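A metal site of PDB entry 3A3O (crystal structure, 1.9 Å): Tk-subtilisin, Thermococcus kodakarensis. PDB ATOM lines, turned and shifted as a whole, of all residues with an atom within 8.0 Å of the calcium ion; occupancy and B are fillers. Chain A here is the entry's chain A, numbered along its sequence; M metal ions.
The calcium ion is bound by the backbone carbonyl oxygen (O) of Leu 95 (2.3 Å).
O of Val 101 is bound to the calcium ion, 2.3 Å away.
O of Ile 99 binds the calcium ion, 2.3 Å away.
OD1 of Asn 97 is bound to the calcium ion (2.4 Å).
The calcium ion is bound by OE1 of Gln 15.
OD1 of Asp 55 is bound to the calcium ion.
The calcium ion is bound by OD2 of Asp 55 (2.5 Å).
The calcium ion has seven donor atoms within binding distance.
O of Asp 98 lies within hydrogen-bond range of N of Gln 15 (3.2 Å).
OD1 of Asn 96 is in hydrogen-bond range of NE2 of Gln 15, at 2.9 Å.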
ATOM      1  N   GLN A  12     -21.560   5.836  -6.336  1.00  0.00           N
ATOM      2  CA  GLN A  12     -22.160   5.267  -7.605  1.00  0.00           C
ATOM      3  C   GLN A  12     -22.679   6.382  -8.509  1.00  0.00           C
ATOM      4  O   GLN A  12     -23.459   7.218  -8.060  1.00  0.00           O
ATOM      5  CB  GLN A  12     -23.297   4.286  -7.295  1.00  0.00           C
ATOM      6  CG  GLN A  12     -22.853   2.925  -6.749  1.00  0.00           C
ATOM      7  CD  GLN A  12     -22.080   2.094  -7.776  1.00  0.00           C
ATOM      8  OE1 GLN A  12     -22.397   2.097  -8.965  1.00  0.00           O
ATOM      9  NE2 GLN A  12     -21.037   1.409  -7.328  1.00  0.00           N
ATOM     10  N   PRO A  13     -22.281   6.379  -9.801  1.00  0.00           N
ATOM     11  CA  PRO A  13     -22.806   7.389 -10.720  1.00  0.00           C
ATOM     12  C   PRO A  13     -24.270   7.168 -11.085  1.00  0.00           C
ATOM     13  O   PRO A  13     -24.761   6.023 -10.990  1.00  0.00           O
ATOM     14  CB  PRO A  13     -21.930   7.228 -11.971  1.00  0.00           C
ATOM     15  CG  PRO A  13     -21.434   5.776 -11.910  1.00  0.00           C
ATOM     16  CD  PRO A  13     -21.346   5.426 -10.436  1.00  0.00           C
ATOM     17  N   ALA A  14     -24.958   8.247 -11.506  1.00  0.00           N
ATOM     18  CA  ALA A  14     -26.324   8.184 -12.039  1.00  0.00           C
ATOM     19  C   ALA A  14     -26.363   7.325 -13.300  1.00  0.00           C
ATOM     20  O   ALA A  14     -25.388   7.314 -14.077  1.00  0.00           O
ATOM     21  CB  ALA A  14     -26.852   9.587 -12.333  1.00  0.00           C
ATOM     22  N   GLN A  15     -27.481   6.621 -13.494  1.00  0.00           N
ATOM     23  CA  GLN A  15     -27.619   5.667 -14.612  1.00  0.00           C
ATOM     24  C   GLN A  15     -27.571   6.334 -15.986  1.00  0.00           C
ATOM     25  O   GLN A  15     -28.216   7.365 -16.213  1.00  0.00           O
ATOM     26  CB  GLN A  15     -28.911   4.850 -14.489  1.00  0.00           C
ATOM     27  CG  GLN A  15     -29.082   3.764 -15.562  1.00  0.00           C
ATOM     28  CD  GLN A  15     -30.203   2.815 -15.272  1.00  0.00           C
ATOM     29  OE1 GLN A  15     -30.047   1.902 -14.458  1.00  0.00           O
ATOM     30  NE2 GLN A  15     -31.352   3.027 -15.916  1.00  0.00           N
ATOM     31  N   THR A  16     -26.774   5.752 -16.901  1.00  0.00           N
ATOM     32  CA  THR A  16     -26.908   6.058 -18.330  1.00  0.00           C
ATOM     33  C   THR A  16     -27.274   4.815 -19.075  1.00  0.00           C
ATOM     34  O   THR A  16     -26.978   3.712 -18.614  1.00  0.00           O
ATOM     35  CB  THR A  16     -25.579   6.348 -19.048  1.00  0.00           C
ATOM     36  OG1 THR A  16     -24.456   6.180 -18.165  1.00  0.00           O
ATOM     37  CG2 THR A  16     -25.616   7.649 -19.821  1.00  0.00           C
ATOM     38  N   HIS A  53     -21.588  -6.463  -7.016  1.00  0.00           N
ATOM     39  CA  HIS A  53     -21.726  -5.174  -7.686  1.00  0.00           C
ATOM     40  C   HIS A  53     -23.154  -4.657  -7.523  1.00  0.00           C
ATOM     41  O   HIS A  53     -24.114  -5.386  -7.771  1.00  0.00           O
ATOM     42  CB  HIS A  53     -21.348  -5.288  -9.166  1.00  0.00           C
ATOM     43  CG  HIS A  53     -21.222  -3.962  -9.851  1.00  0.00           C
ATOM     44  ND1 HIS A  53     -20.068  -3.560 -10.473  1.00  0.00           N
ATOM     45  CD2 HIS A  53     -22.105  -2.952  -9.997  1.00  0.00           C
ATOM     46  CE1 HIS A  53     -20.247  -2.362 -11.005  1.00  0.00           C
ATOM     47  NE2 HIS A  53     -21.471  -1.958 -10.713  1.00  0.00           N
ATOM     48  N   PRO A  54     -23.337  -3.410  -7.046  1.00  0.00           N
ATOM     49  CA  PRO A  54     -24.713  -2.894  -6.834  1.00  0.00           C
ATOM     50  C   PRO A  54     -25.567  -2.863  -8.101  1.00  0.00           C
ATOM     51  O   PRO A  54     -26.813  -2.878  -8.034  1.00  0.00           O
ATOM     52  CB  PRO A  54     -24.491  -1.451  -6.336  1.00  0.00           C
ATOM     53  CG  PRO A  54     -23.109  -1.444  -5.770  1.00  0.00           C
ATOM     54  CD  PRO A  54     -22.303  -2.437  -6.615  1.00  0.00           C
ATOM     55  N   ASP A  55     -24.928  -2.813  -9.265  1.00  0.00           N
ATOM     56  CA  ASP A  55     -25.702  -2.797 -10.523  1.00  0.00           C
ATOM     57  C   ASP A  55     -25.883  -4.173 -11.164  1.00  0.00           C
ATOM     58  O   ASP A  55     -26.407  -4.267 -12.285  1.00  0.00           O
ATOM     59  CB  ASP A  55     -25.135  -1.797 -11.546  1.00  0.00           C
ATOM     60  CG  ASP A  55     -26.249  -1.036 -12.266  1.00  0.00           C
ATOM     61  OD1 ASP A  55     -27.372  -0.924 -11.722  1.00  0.00           O
ATOM     62  OD2 ASP A  55     -26.041  -0.514 -13.377  1.00  0.00           O
ATOM     63  N   LEU A  56     -25.455  -5.222 -10.435  1.00  0.00           N
ATOM     64  CA  LEU A  56     -25.554  -6.614 -10.901  1.00  0.00           C
ATOM     65  C   LEU A  56     -26.190  -7.578  -9.914  1.00  0.00           C
ATOM     66  O   LEU A  56     -26.809  -8.587 -10.309  1.00  0.00           O
ATOM     67  CB  LEU A  56     -24.163  -7.161 -11.241  1.00  0.00           C
ATOM     68  CG  LEU A  56     -23.331  -6.571 -12.395  1.00  0.00           C
ATOM     69  CD1 LEU A  56     -22.103  -7.433 -12.544  1.00  0.00           C
ATOM     70  CD2 LEU A  56     -24.107  -6.543 -13.697  1.00  0.00           C
ATOM     71  N   ALA A  93     -27.273  -7.698 -18.434  1.00  0.00           N
ATOM     72  CA  ALA A  93     -28.204  -7.755 -17.282  1.00  0.00           C
ATOM     73  C   ALA A  93     -27.996  -6.708 -16.201  1.00  0.00           C
ATOM     74  O   ALA A  93     -28.539  -6.864 -15.078  1.00  0.00           O
ATOM     75  CB  ALA A  93     -28.149  -9.132 -16.667  1.00  0.00           C
ATOM     76  N   ALA A  94     -27.239  -5.640 -16.509  1.00  0.00           N
ATOM     77  CA  ALA A  94     -27.136  -4.542 -15.517  1.00  0.00           C
ATOM     78  C   ALA A  94     -28.554  -4.031 -15.188  1.00  0.00           C
ATOM     79  O   ALA A  94     -29.400  -3.911 -16.075  1.00  0.00           O
ATOM     80  CB  ALA A  94     -26.261  -3.417 -16.032  1.00  0.00           C
ATOM     81  N   LEU A  95     -28.815  -3.744 -13.912  1.00  0.00           N
ATOM     82  CA  LEU A  95     -30.172  -3.435 -13.454  1.00  0.00           C
ATOM     83  C   LEU A  95     -30.648  -2.062 -13.929  1.00  0.00           C
ATOM     84  O   LEU A  95     -29.848  -1.109 -14.036  1.00  0.00           O
ATOM     85  CB  LEU A  95     -30.188  -3.509 -11.918  1.00  0.00           C
ATOM     86  CG  LEU A  95     -29.966  -4.913 -11.348  1.00  0.00           C
ATOM     87  CD1 LEU A  95     -29.262  -4.893  -9.960  1.00  0.00           C
ATOM     88  CD2 LEU A  95     -31.292  -5.666 -11.259  1.00  0.00           C
ATOM     89  N   ASN A  96     -31.942  -1.967 -14.217  1.00  0.00           N
ATOM     90  CA  ASN A  96     -32.564  -0.699 -14.585  1.00  0.00           C
ATOM     91  C   ASN A  96     -32.997  -0.008 -13.286  1.00  0.00           C
ATOM     92  O   ASN A  96     -33.982  -0.404 -12.665  1.00  0.00           O
ATOM     93  CB  ASN A  96     -33.763  -0.944 -15.475  1.00  0.00           C
ATOM     94  CG  ASN A  96     -34.332   0.339 -16.067  1.00  0.00           C
ATOM     95  OD1 ASN A  96     -33.789   1.421 -15.840  1.00  0.00           O
ATOM     96  ND2 ASN A  96     -35.411   0.222 -16.820  1.00  0.00           N
ATOM     97  N   ASN A  97     -32.229   0.991 -12.866  1.00  0.00           N
ATOM     98  CA  ASN A  97     -32.416   1.619 -11.555  1.00  0.00           C
ATOM     99  C   ASN A  97     -31.859   3.042 -11.609  1.00  0.00           C
ATOM    100  O   ASN A  97     -31.805   3.641 -12.678  1.00  0.00           O
ATOM    101  CB  ASN A  97     -31.745   0.751 -10.442  1.00  0.00           C
ATOM    102  CG  ASN A  97     -30.251   0.448 -10.713  1.00  0.00           C
ATOM    103  OD1 ASN A  97     -29.612   1.065 -11.574  1.00  0.00           O
ATOM    104  ND2 ASN A  97     -29.681  -0.487  -9.939  1.00  0.00           N
ATOM    105  N   ASP A  98     -31.371   3.546 -10.483  1.00  0.00           N
ATOM    106  CA  ASP A  98     -30.880   4.912 -10.446  1.00  0.00           C
ATOM    107  C   ASP A  98     -29.389   5.070 -10.677  1.00  0.00           C
ATOM    108  O   ASP A  98     -28.885   6.185 -10.651  1.00  0.00           O
ATOM    109  CB  ASP A  98     -31.308   5.594  -9.124  1.00  0.00           C
ATOM    110  CG  ASP A  98     -32.816   5.625  -8.949  1.00  0.00           C
ATOM    111  OD1 ASP A  98     -33.536   6.018  -9.912  1.00  0.00           O
ATOM    112  OD2 ASP A  98     -33.307   5.253  -7.849  1.00  0.00           O
ATOM    113  N   ILE A  99     -28.686   3.964 -10.910  1.00  0.00           N
ATOM    114  CA  ILE A  99     -27.223   3.969 -10.957  1.00  0.00           C
ATOM    115  C   ILE A  99     -26.605   3.256 -12.169  1.00  0.00           C
ATOM    116  O   ILE A  99     -27.213   2.364 -12.748  1.00  0.00           O
ATOM    117  CB  ILE A  99     -26.605   3.336  -9.671  1.00  0.00           C
ATOM    118  CG1 ILE A  99     -27.143   1.904  -9.451  1.00  0.00           C
ATOM    119  CG2 ILE A  99     -26.907   4.224  -8.418  1.00  0.00           C
ATOM    120  CD1 ILE A  99     -26.270   1.062  -8.542  1.00  0.00           C
ATOM    121  N   GLY A 100     -25.400   3.658 -12.535  1.00  0.00           N
ATOM    122  CA  GLY A 100     -24.535   2.836 -13.364  1.00  0.00           C
ATOM    123  C   GLY A 100     -24.983   2.744 -14.800  1.00  0.00           C
ATOM    124  O   GLY A 100     -25.051   3.759 -15.501  1.00  0.00           O
ATOM    125  N   VAL A 101     -25.249   1.535 -15.281  1.00  0.00           N
ATOM    126  CA  VAL A 101     -25.654   1.352 -16.677  1.00  0.00           C
ATOM    127  C   VAL A 101     -26.949   0.534 -16.687  1.00  0.00           C
ATOM    128  O   VAL A 101     -27.628   0.454 -15.657  1.00  0.00           O
ATOM    129  CB  VAL A 101     -24.508   0.720 -17.517  1.00  0.00           C
ATOM    130  CG1 VAL A 101     -23.340   1.710 -17.697  1.00  0.00           C
ATOM    131  CG2 VAL A 101     -24.009  -0.635 -16.893  1.00  0.00           C
ATOM    132  N   VAL A 102     -27.326  -0.063 -17.817  1.00  0.00           N
ATOM    133  CA  VAL A 102     -28.498  -0.932 -17.874  1.00  0.00           C
ATOM    134  C   VAL A 102     -28.242  -1.944 -18.991  1.00  0.00           C
ATOM    135  O   VAL A 102     -27.703  -1.577 -20.021  1.00  0.00           O
ATOM    136  CB  VAL A 102     -29.824  -0.135 -18.095  1.00  0.00           C
ATOM    137  CG1 VAL A 102     -29.827   0.662 -19.426  1.00  0.00           C
ATOM    138  CG2 VAL A 102     -31.052  -1.026 -17.957  1.00  0.00           C
ATOM    139  N   GLY A 103     -28.631  -3.206 -18.760  1.00  0.00           N
ATOM    140  CA  GLY A 103     -28.380  -4.281 -19.738  1.00  0.00           C
ATOM    141  C   GLY A 103     -29.481  -4.317 -20.777  1.00  0.00           C
ATOM    142  O   GLY A 103     -30.500  -3.626 -20.661  1.00  0.00           O
ATOM    143  N   PRO A 106     -32.510  -6.208 -18.512  1.00  0.00           N
ATOM    144  CA  PRO A 106     -32.135  -5.798 -17.181  1.00  0.00           C
ATOM    145  C   PRO A 106     -32.810  -6.542 -16.008  1.00  0.00           C
ATOM    146  O   PRO A 106     -32.438  -6.275 -14.868  1.00  0.00           O
ATOM    147  CB  PRO A 106     -32.444  -4.294 -17.172  1.00  0.00           C
ATOM    148  CG  PRO A 106     -33.436  -4.057 -18.193  1.00  0.00           C
ATOM    149  CD  PRO A 106     -33.265  -5.166 -19.230  1.00  0.00           C
ATOM    150  N   THR A 242     -20.402  -2.558 -16.498  1.00  0.00           N
ATOM    151  CA  THR A 242     -19.906  -2.815 -15.154  1.00  0.00           C
ATOM    152  C   THR A 242     -18.456  -3.364 -15.187  1.00  0.00           C
ATOM    153  O   THR A 242     -18.039  -4.023 -16.153  1.00  0.00           O
ATOM    154  CB  THR A 242     -20.861  -3.778 -14.406  1.00  0.00           C
ATOM    155  OG1 THR A 242     -21.199  -4.864 -15.284  1.00  0.00           O
ATOM    156  CG2 THR A 242     -22.188  -3.027 -14.048  1.00  0.00           C
ATOM    157  N   TYR A 248     -17.122   0.829 -13.308  1.00  0.00           N
ATOM    158  CA  TYR A 248     -17.577   0.794 -14.717  1.00  0.00           C
ATOM    159  C   TYR A 248     -16.342   0.987 -15.581  1.00  0.00           C
ATOM    160  O   TYR A 248     -15.348   1.583 -15.126  1.00  0.00           O
ATOM    161  CB  TYR A 248     -18.691   1.861 -14.997  1.00  0.00           C
ATOM    162  CG  TYR A 248     -19.831   1.690 -14.051  1.00  0.00           C
ATOM    163  CD1 TYR A 248     -19.787   2.285 -12.777  1.00  0.00           C
ATOM    164  CD2 TYR A 248     -20.888   0.825 -14.343  1.00  0.00           C
ATOM    165  CE1 TYR A 248     -20.763   2.061 -11.849  1.00  0.00           C
ATOM    166  CE2 TYR A 248     -21.886   0.599 -13.423  1.00  0.00           C
ATOM    167  CZ  TYR A 248     -21.816   1.221 -12.167  1.00  0.00           C
ATOM    168  OH  TYR A 248     -22.796   0.989 -11.237  1.00  0.00           O
HETATM  169 CA    CA M   1     -28.350   0.496 -13.479  1.00  0.00          CA
